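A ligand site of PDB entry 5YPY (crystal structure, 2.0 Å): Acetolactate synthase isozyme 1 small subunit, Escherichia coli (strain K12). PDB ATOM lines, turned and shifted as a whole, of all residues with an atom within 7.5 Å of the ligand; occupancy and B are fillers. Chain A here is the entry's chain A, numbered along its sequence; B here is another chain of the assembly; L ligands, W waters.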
ATOM      1  N   VAL A  17      10.260 -17.494  34.601  1.00  0.00           N
ATOM      2  CA  VAL A  17      11.612 -16.922  34.543  1.00  0.00           C
ATOM      3  C   VAL A  17      11.610 -15.651  33.716  1.00  0.00           C
ATOM      4  O   VAL A  17      10.680 -15.365  32.954  1.00  0.00           O
ATOM      5  CB  VAL A  17      12.612 -17.926  33.970  1.00  0.00           C
ATOM      6  CG1 VAL A  17      12.621 -19.208  34.793  1.00  0.00           C
ATOM      7  CG2 VAL A  17      12.254 -18.215  32.505  1.00  0.00           C
ATOM      8  N   ARG A  18      12.683 -14.874  33.875  1.00  0.00           N
ATOM      9  CA  ARG A  18      12.961 -13.739  32.989  1.00  0.00           C
ATOM     10  C   ARG A  18      13.405 -14.232  31.608  1.00  0.00           C
ATOM     11  O   ARG A  18      14.140 -15.223  31.479  1.00  0.00           O
ATOM     12  CB  ARG A  18      14.071 -12.875  33.583  1.00  0.00           C
ATOM     13  CG  ARG A  18      13.630 -12.031  34.741  1.00  0.00           C
ATOM     14  CD  ARG A  18      14.688 -11.974  35.825  1.00  0.00           C
ATOM     15  NE  ARG A  18      14.168 -11.380  37.055  1.00  0.00           N
ATOM     16  CZ  ARG A  18      14.899 -10.757  37.968  1.00  0.00           C
ATOM     17  NH1 ARG A  18      16.222 -10.630  37.806  1.00  0.00           N
ATOM     18  NH2 ARG A  18      14.321 -10.254  39.047  1.00  0.00           N
ATOM     19  N   ASN A  19      12.950 -13.552  30.558  1.00  0.00           N
ATOM     20  CA  ASN A  19      13.253 -14.016  29.207  1.00  0.00           C
ATOM     21  C   ASN A  19      14.490 -13.281  28.692  1.00  0.00           C
ATOM     22  O   ASN A  19      14.421 -12.375  27.860  1.00  0.00           O
ATOM     23  CB  ASN A  19      12.059 -13.807  28.289  1.00  0.00           C
ATOM     24  CG  ASN A  19      12.225 -14.515  26.960  1.00  0.00           C
ATOM     25  OD1 ASN A  19      13.145 -15.340  26.770  1.00  0.00           O
ATOM     26  ND2 ASN A  19      11.337 -14.192  26.030  1.00  0.00           N
ATOM     27  N   HIS A  20      15.634 -13.662  29.261  1.00  0.00           N
ATOM     28  CA  HIS A  20      16.943 -13.050  29.091  1.00  0.00           C
ATOM     29  C   HIS A  20      17.908 -14.152  28.693  1.00  0.00           C
ATOM     30  O   HIS A  20      17.670 -15.319  28.993  1.00  0.00           O
ATOM     31  CB  HIS A  20      17.467 -12.405  30.384  1.00  0.00           C
ATOM     32  CG  HIS A  20      16.635 -11.264  30.871  1.00  0.00           C
ATOM     33  ND1 HIS A  20      15.653 -10.669  30.119  1.00  0.00           N
ATOM     34  CD2 HIS A  20      16.670 -10.587  32.049  1.00  0.00           C
ATOM     35  CE1 HIS A  20      15.107  -9.684  30.804  1.00  0.00           C
ATOM     36  NE2 HIS A  20      15.700  -9.608  31.973  1.00  0.00           N
ATOM     37  N   PRO A  21      18.980 -13.820  27.976  1.00  0.00           N
ATOM     38  CA  PRO A  21      19.963 -14.850  27.637  1.00  0.00           C
ATOM     39  C   PRO A  21      20.583 -15.428  28.907  1.00  0.00           C
ATOM     40  O   PRO A  21      20.807 -14.722  29.896  1.00  0.00           O
ATOM     41  CB  PRO A  21      21.009 -14.087  26.817  1.00  0.00           C
ATOM     42  CG  PRO A  21      20.364 -12.862  26.361  1.00  0.00           C
ATOM     43  CD  PRO A  21      19.179 -12.578  27.235  1.00  0.00           C
ATOM     44  N   GLY A  22      20.854 -16.732  28.870  1.00  0.00           N
ATOM     45  CA  GLY A  22      21.527 -17.405  29.964  1.00  0.00           C
ATOM     46  C   GLY A  22      20.622 -18.076  30.961  1.00  0.00           C
ATOM     47  O   GLY A  22      21.087 -18.932  31.732  1.00  0.00           O
ATOM     48  N   VAL A  23      19.338 -17.741  30.984  1.00  0.00           N
ATOM     49  CA  VAL A  23      18.511 -18.225  32.078  1.00  0.00           C
ATOM     50  C   VAL A  23      18.410 -19.738  32.018  1.00  0.00           C
ATOM     51  O   VAL A  23      18.566 -20.424  33.044  1.00  0.00           O
ATOM     52  CB  VAL A  23      17.133 -17.547  32.066  1.00  0.00           C
ATOM     53  CG1 VAL A  23      16.227 -18.250  33.027  1.00  0.00           C
ATOM     54  CG2 VAL A  23      17.270 -16.076  32.399  1.00  0.00           C
ATOM     55  N   MET A  24      18.172 -20.301  30.836  1.00  0.00           N
ATOM     56  CA  MET A  24      17.980 -21.743  30.780  1.00  0.00           C
ATOM     57  C   MET A  24      19.285 -22.446  31.135  1.00  0.00           C
ATOM     58  O   MET A  24      19.251 -23.556  31.656  1.00  0.00           O
ATOM     59  CB  MET A  24      17.491 -22.195  29.392  1.00  0.00           C
ATOM     60  CG  MET A  24      17.468 -23.713  29.202  1.00  0.00           C
ATOM     61  SD  MET A  24      15.966 -24.524  30.012  1.00  0.00           S
ATOM     62  CE  MET A  24      14.714 -23.400  29.534  1.00  0.00           C
ATOM     63  N   THR A  25      20.440 -21.831  30.843  1.00  0.00           N
ATOM     64  CA  THR A  25      21.717 -22.453  31.146  1.00  0.00           C
ATOM     65  C   THR A  25      21.915 -22.534  32.668  1.00  0.00           C
ATOM     66  O   THR A  25      22.335 -23.578  33.189  1.00  0.00           O
ATOM     67  CB  THR A  25      22.855 -21.693  30.481  1.00  0.00           C
ATOM     68  OG1 THR A  25      22.704 -21.724  29.035  1.00  0.00           O
ATOM     69  CG2 THR A  25      24.216 -22.310  30.876  1.00  0.00           C
ATOM     70  N   HIS A  26      21.556 -21.459  33.380  1.00  0.00           N
ATOM     71  CA  HIS A  26      21.584 -21.483  34.845  1.00  0.00           C
ATOM     72  C   HIS A  26      20.651 -22.554  35.421  1.00  0.00           C
ATOM     73  O   HIS A  26      20.996 -23.234  36.393  1.00  0.00           O
ATOM     74  CB  HIS A  26      21.228 -20.104  35.391  1.00  0.00           C
ATOM     75  CG  HIS A  26      22.217 -19.050  35.011  1.00  0.00           C
ATOM     76  ND1 HIS A  26      21.873 -17.726  34.861  1.00  0.00           N
ATOM     77  CD2 HIS A  26      23.541 -19.129  34.755  1.00  0.00           C
ATOM     78  CE1 HIS A  26      22.943 -17.022  34.535  1.00  0.00           C
ATOM     79  NE2 HIS A  26      23.973 -17.854  34.468  1.00  0.00           N
ATOM     80  N   CYS A  43       9.592 -24.540  26.874  1.00  0.00           N
ATOM     81  CA  CYS A  43       9.815 -23.157  27.263  1.00  0.00           C
ATOM     82  C   CYS A  43       9.034 -22.273  26.297  1.00  0.00           C
ATOM     83  O   CYS A  43       9.284 -22.300  25.092  1.00  0.00           O
ATOM     84  CB  CYS A  43      11.295 -22.759  27.238  1.00  0.00           C
ATOM     85  SG  CYS A  43      11.534 -20.958  27.545  1.00  0.00           S
ATOM     86  N   LEU A  44       8.079 -21.488  26.843  1.00  0.00           N
ATOM     87  CA  LEU A  44       7.325 -20.559  26.044  1.00  0.00           C
ATOM     88  C   LEU A  44       7.328 -19.160  26.639  1.00  0.00           C
ATOM     89  O   LEU A  44       7.266 -18.993  27.860  1.00  0.00           O
ATOM     90  CB  LEU A  44       5.899 -21.043  25.871  1.00  0.00           C
ATOM     91  CG  LEU A  44       5.660 -22.361  25.130  1.00  0.00           C
ATOM     92  CD1 LEU A  44       4.264 -22.855  25.449  1.00  0.00           C
ATOM     93  CD2 LEU A  44       5.857 -22.026  23.552  1.00  0.00           C
ATOM     94  N   PRO A  45       7.437 -18.124  25.806  1.00  0.00           N
ATOM     95  CA  PRO A  45       7.373 -16.751  26.323  1.00  0.00           C
ATOM     96  C   PRO A  45       5.953 -16.480  26.756  1.00  0.00           C
ATOM     97  O   PRO A  45       5.008 -17.077  26.250  1.00  0.00           O
ATOM     98  CB  PRO A  45       7.746 -15.865  25.124  1.00  0.00           C
ATOM     99  CG  PRO A  45       8.097 -16.795  24.034  1.00  0.00           C
ATOM    100  CD  PRO A  45       7.595 -18.172  24.345  1.00  0.00           C
ATOM    101  N   LYS A  51       8.857 -12.211  30.490  1.00  0.00           N
ATOM    102  CA  LYS A  51       9.007 -13.465  31.206  1.00  0.00           C
ATOM    103  C   LYS A  51       8.568 -14.633  30.346  1.00  0.00           C
ATOM    104  O   LYS A  51       7.866 -14.477  29.339  1.00  0.00           O
ATOM    105  CB  LYS A  51       8.199 -13.447  32.522  1.00  0.00           C
ATOM    106  CG  LYS A  51       8.732 -12.432  33.557  1.00  0.00           C
ATOM    107  CD  LYS A  51       7.984 -12.471  34.875  1.00  0.00           C
ATOM    108  CE  LYS A  51       8.317 -11.259  35.757  1.00  0.00           C
ATOM    109  NZ  LYS A  51       7.698  -9.968  35.288  1.00  0.00           N
ATOM    110  N   SER A  52       9.006 -15.815  30.766  1.00  0.00           N
ATOM    111  CA  SER A  52       8.668 -17.067  30.100  1.00  0.00           C
ATOM    112  C   SER A  52       8.268 -18.078  31.154  1.00  0.00           C
ATOM    113  O   SER A  52       8.653 -17.976  32.331  1.00  0.00           O
ATOM    114  CB  SER A  52       9.878 -17.642  29.310  1.00  0.00           C
ATOM    115  OG  SER A  52      10.258 -16.695  28.345  1.00  0.00           O
ATOM    116  N   HIS A  53       7.585 -19.118  30.684  1.00  0.00           N
ATOM    117  CA  HIS A  53       7.481 -20.360  31.432  1.00  0.00           C
ATOM    118  C   HIS A  53       8.453 -21.379  30.896  1.00  0.00           C
ATOM    119  O   HIS A  53       8.628 -21.508  29.684  1.00  0.00           O
ATOM    120  CB  HIS A  53       6.074 -20.923  31.338  1.00  0.00           C
ATOM    121  CG  HIS A  53       5.054 -20.055  31.976  1.00  0.00           C
ATOM    122  ND1 HIS A  53       3.918 -19.628  31.325  1.00  0.00           N
ATOM    123  CD2 HIS A  53       5.039 -19.460  33.190  1.00  0.00           C
ATOM    124  CE1 HIS A  53       3.219 -18.851  32.121  1.00  0.00           C
ATOM    125  NE2 HIS A  53       3.875 -18.733  33.269  1.00  0.00           N
ATOM    126  N   ILE A  54       9.079 -22.115  31.810  1.00  0.00           N
ATOM    127  CA  ILE A  54       9.770 -23.331  31.508  1.00  0.00           C
ATOM    128  C   ILE A  54       9.078 -24.452  32.274  1.00  0.00           C
ATOM    129  O   ILE A  54       8.989 -24.402  33.518  1.00  0.00           O
ATOM    130  CB  ILE A  54      11.250 -23.234  31.953  1.00  0.00           C
ATOM    131  CG1 ILE A  54      11.882 -21.999  31.301  1.00  0.00           C
ATOM    132  CG2 ILE A  54      11.913 -24.505  31.700  1.00  0.00           C
ATOM    133  CD1 ILE A  54      13.321 -21.611  31.827  1.00  0.00           C
ATOM    134  N   MET B  24      21.908 -30.294  27.882  1.00  0.00           N
ATOM    135  CA  MET B  24      21.195 -29.053  27.597  1.00  0.00           C
ATOM    136  C   MET B  24      21.914 -27.841  28.174  1.00  0.00           C
ATOM    137  O   MET B  24      21.850 -26.752  27.603  1.00  0.00           O
ATOM    138  CB  MET B  24      19.751 -29.158  28.127  1.00  0.00           C
ATOM    139  CG  MET B  24      18.916 -27.972  27.883  1.00  0.00           C
ATOM    140  SD  MET B  24      18.512 -27.918  26.108  1.00  0.00           S
ATOM    141  CE  MET B  24      17.229 -26.714  26.155  1.00  0.00           C
ATOM    142  N   CYS B  28      22.731 -24.744  25.611  1.00  0.00           N
ATOM    143  CA  CYS B  28      22.263 -23.394  25.910  1.00  0.00           C
ATOM    144  C   CYS B  28      23.415 -22.484  26.290  1.00  0.00           C
ATOM    145  O   CYS B  28      23.371 -21.272  26.026  1.00  0.00           O
ATOM    146  CB  CYS B  28      21.165 -23.442  27.017  1.00  0.00           C
ATOM    147  SG  CYS B  28      19.643 -24.151  26.314  1.00  0.00           S
ATOM    148  N   PHE B  31      24.627 -20.350  23.550  1.00  0.00           N
ATOM    149  CA  PHE B  31      23.843 -19.150  23.290  1.00  0.00           C
ATOM    150  C   PHE B  31      24.107 -18.122  24.375  1.00  0.00           C
ATOM    151  O   PHE B  31      24.338 -16.943  24.079  1.00  0.00           O
ATOM    152  CB  PHE B  31      22.333 -19.488  23.220  1.00  0.00           C
ATOM    153  CG  PHE B  31      21.962 -20.337  22.035  1.00  0.00           C
ATOM    154  CD1 PHE B  31      21.981 -21.728  22.107  1.00  0.00           C
ATOM    155  CD2 PHE B  31      21.609 -19.758  20.840  1.00  0.00           C
ATOM    156  CE1 PHE B  31      21.663 -22.520  20.986  1.00  0.00           C
ATOM    157  CE2 PHE B  31      21.278 -20.549  19.714  1.00  0.00           C
ATOM    158  CZ  PHE B  31      21.307 -21.938  19.826  1.00  0.00           C
ATOM    159  N   ALA B  32      24.118 -18.556  25.639  1.00  0.00           N
ATOM    160  CA  ALA B  32      24.388 -17.638  26.743  1.00  0.00           C
ATOM    161  C   ALA B  32      25.728 -16.920  26.558  1.00  0.00           C
ATOM    162  O   ALA B  32      25.810 -15.699  26.770  1.00  0.00           O
ATOM    163  CB  ALA B  32      24.381 -18.421  28.068  1.00  0.00           C
ATOM    164  N   PHE B  36      22.746 -14.378  23.382  1.00  0.00           N
ATOM    165  CA  PHE B  36      21.808 -14.720  22.323  1.00  0.00           C
ATOM    166  C   PHE B  36      20.615 -15.373  22.984  1.00  0.00           C
ATOM    167  O   PHE B  36      20.719 -16.490  23.489  1.00  0.00           O
ATOM    168  CB  PHE B  36      22.458 -15.682  21.334  1.00  0.00           C
ATOM    169  CG  PHE B  36      21.706 -15.827  20.011  1.00  0.00           C
ATOM    170  CD1 PHE B  36      20.334 -15.647  19.931  1.00  0.00           C
ATOM    171  CD2 PHE B  36      22.387 -16.135  18.858  1.00  0.00           C
ATOM    172  CE1 PHE B  36      19.660 -15.756  18.725  1.00  0.00           C
ATOM    173  CE2 PHE B  36      21.722 -16.244  17.647  1.00  0.00           C
ATOM    174  CZ  PHE B  36      20.347 -16.054  17.581  1.00  0.00           C
ATOM    175  N   ASN B  37      19.471 -14.725  22.928  1.00  0.00           N
ATOM    176  CA  ASN B  37      18.336 -15.240  23.663  1.00  0.00           C
ATOM    177  C   ASN B  37      17.671 -16.388  22.888  1.00  0.00           C
ATOM    178  O   ASN B  37      17.649 -16.394  21.658  1.00  0.00           O
ATOM    179  CB  ASN B  37      17.379 -14.095  23.933  1.00  0.00           C
ATOM    180  CG  ASN B  37      16.259 -14.483  24.832  1.00  0.00           C
ATOM    181  OD1 ASN B  37      16.491 -14.818  25.993  1.00  0.00           O
ATOM    182  ND2 ASN B  37      15.034 -14.473  24.300  1.00  0.00           N
ATOM    183  N   VAL B  38      17.170 -17.371  23.634  1.00  0.00           N
ATOM    184  CA  VAL B  38      16.375 -18.473  23.075  1.00  0.00           C
ATOM    185  C   VAL B  38      14.901 -18.223  23.367  1.00  0.00           C
ATOM    186  O   VAL B  38      14.509 -18.020  24.513  1.00  0.00           O
ATOM    187  CB  VAL B  38      16.836 -19.821  23.649  1.00  0.00           C
ATOM    188  CG1 VAL B  38      15.877 -20.908  23.188  1.00  0.00           C
ATOM    189  CG2 VAL B  38      18.291 -20.089  23.153  1.00  0.00           C
ATOM    190  N   GLU B  39      14.068 -18.214  22.325  1.00  0.00           N
ATOM    191  CA  GLU B  39      12.691 -17.786  22.557  1.00  0.00           C
ATOM    192  C   GLU B  39      11.779 -18.941  22.917  1.00  0.00           C
ATOM    193  O   GLU B  39      10.829 -18.752  23.656  1.00  0.00           O
ATOM    194  CB  GLU B  39      12.137 -17.075  21.310  1.00  0.00           C
ATOM    195  CG  GLU B  39      12.946 -15.852  20.847  1.00  0.00           C
ATOM    196  CD  GLU B  39      12.995 -14.738  21.910  1.00  0.00           C
ATOM    197  OE1 GLU B  39      12.095 -14.710  22.790  1.00  0.00           O
ATOM    198  OE2 GLU B  39      13.927 -13.906  21.829  1.00  0.00           O
ATOM    199  N   GLY B  40      12.066 -20.118  22.421  1.00  0.00           N
ATOM    200  CA  GLY B  40      11.223 -21.280  22.587  1.00  0.00           C
ATOM    201  C   GLY B  40      12.151 -22.479  22.602  1.00  0.00           C
ATOM    202  O   GLY B  40      13.160 -22.522  21.891  1.00  0.00           O
ATOM    203  N   ILE B  41      11.796 -23.456  23.429  1.00  0.00           N
ATOM    204  CA  ILE B  41      12.437 -24.738  23.503  1.00  0.00           C
ATOM    205  C   ILE B  41      11.402 -25.830  23.613  1.00  0.00           C
ATOM    206  O   ILE B  41      10.462 -25.749  24.423  1.00  0.00           O
ATOM    207  CB  ILE B  41      13.334 -24.805  24.748  1.00  0.00           C
ATOM    208  CG1 ILE B  41      14.339 -23.667  24.701  1.00  0.00           C
ATOM    209  CG2 ILE B  41      14.028 -26.236  24.815  1.00  0.00           C
ATOM    210  CD1 ILE B  41      15.254 -23.625  25.971  1.00  0.00           C
HETATM  211  N1  LIG L   1      15.282 -17.086  27.001  1.00  0.00           N
HETATM  212  C1  LIG L   1      15.931 -17.775  28.118  1.00  0.00           C
HETATM  213  C2  LIG L   1      17.333 -18.234  27.704  1.00  0.00           C
HETATM  214  O1  LIG L   1      17.711 -18.023  26.526  1.00  0.00           O
HETATM  215  C3  LIG L   1      15.082 -18.951  28.603  1.00  0.00           C
HETATM  216  C4  LIG L   1      13.680 -18.469  29.075  1.00  0.00           C
HETATM  217  C5  LIG L   1      14.937 -20.004  27.512  1.00  0.00           C
HETATM  218  O2  LIG L   1      18.090 -18.840  28.506  1.00  0.00           O
HETATM  219  O   HOH W   1      20.550 -19.867  28.137  1.00  0.00           O
HETATM  220  O   HOH W   2      20.129 -17.914  25.981  1.00  0.00           O
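N of Met 24 of chain A is in hydrogen-bond range of O2 of the ligand. An oxygen (O1) of the ligand lies within hydrogen-bond range of the backbone NH (N) of Val 38 of chain B. OD1 of Asn 37 of chain B lies within hydrogen-bond range of N1 of the ligand, 2.8 Å away. The side-chain amide oxygen (OD1) of Asn 19 lies within hydrogen-bond range of a nitrogen (N1) of the ligand (2.8 Å). An oxygen (O2) of the ligand sits at hydrogen-bond distance from the backbone NH (N) of Gly 22, 3.5 Å away. O of Val 38 of chain B sits at hydrogen-bond distance from N1 of the ligand, 2.8 Å away. The backbone NH of Val 23 lies within hydrogen-bond range of an oxygen (O2) of the ligand (3.0 Å).
The side-chain amide oxygen (OD1) of Asn 37 of chain B sits close to the backbone carbonyl oxygen (O) of His 20, at 3.3 Å. The backbone NH of Cys 43 is in hydrogen-bond range of the backbone carbonyl oxygen of Ile 41 of chain B. ND2 of Asn 19 sits at hydrogen-bond distance from OE1 of Glu 39 of chain B. The side-chain sulfur (SG) of Cys 43 sits close to the backbone carbonyl oxygen (O) of His 53. ND2 of Asn 37 of chain B sits at hydrogen-bond distance from OD1 of Asn 19 (3.2 Å). The side-chain amide nitrogen (ND2) of Asn 37 of chain B lies within hydrogen-bond range of the side-chain carboxylate (OE2) of Glu 39 of chain B, 2.8 Å away. The backbone NH of Ser 52 lies within hydrogen-bond range of the backbone carbonyl oxygen of Val 17. The backbone carbonyl oxygen (O) of Gly 22 sits at hydrogen-bond distance from a ring nitrogen (ND1) of His 26.
Residues that only touch the ligand: Val 17 (3.7 Å), His 20 (3.1 Å), Cys 43 (3.5 Å), Ser 52 (3.9 Å) and Ile 41 of chain B (3.9 Å). Hydrophobic or aromatic side chains that line the ligand: Val 17, Val 23, Met 24 of chain A, Val 38 of chain B and Ile 41 of chain B. Within 4 Å of the ligand: Val 17, Asn 19, His 20, Gly 22, Val 23, Met 24 of chain A, Cys 43, Ser 52, Asn 37 of chain B, Val 38 of chain B and Ile 41 of chain B. The nearest printed residue that does not touch the ligand is Pro 21 (4.05 Å).
Water W2 lies within hydrogen-bond range of an oxygen (O1) of the ligand (2.5 Å), the backbone carbonyl oxygen (O) of Phe 36 of chain B (2.9 Å) and the backbone NH (N) of Gly 22 (3.2 Å). Water W1 lies within hydrogen-bond range of an oxygen (O2) of the ligand (2.7 Å), the side-chain hydroxyl (OG1) of Thr 25 (3.0 Å) and the backbone NH (N) of Gly 22 (3.2 Å).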
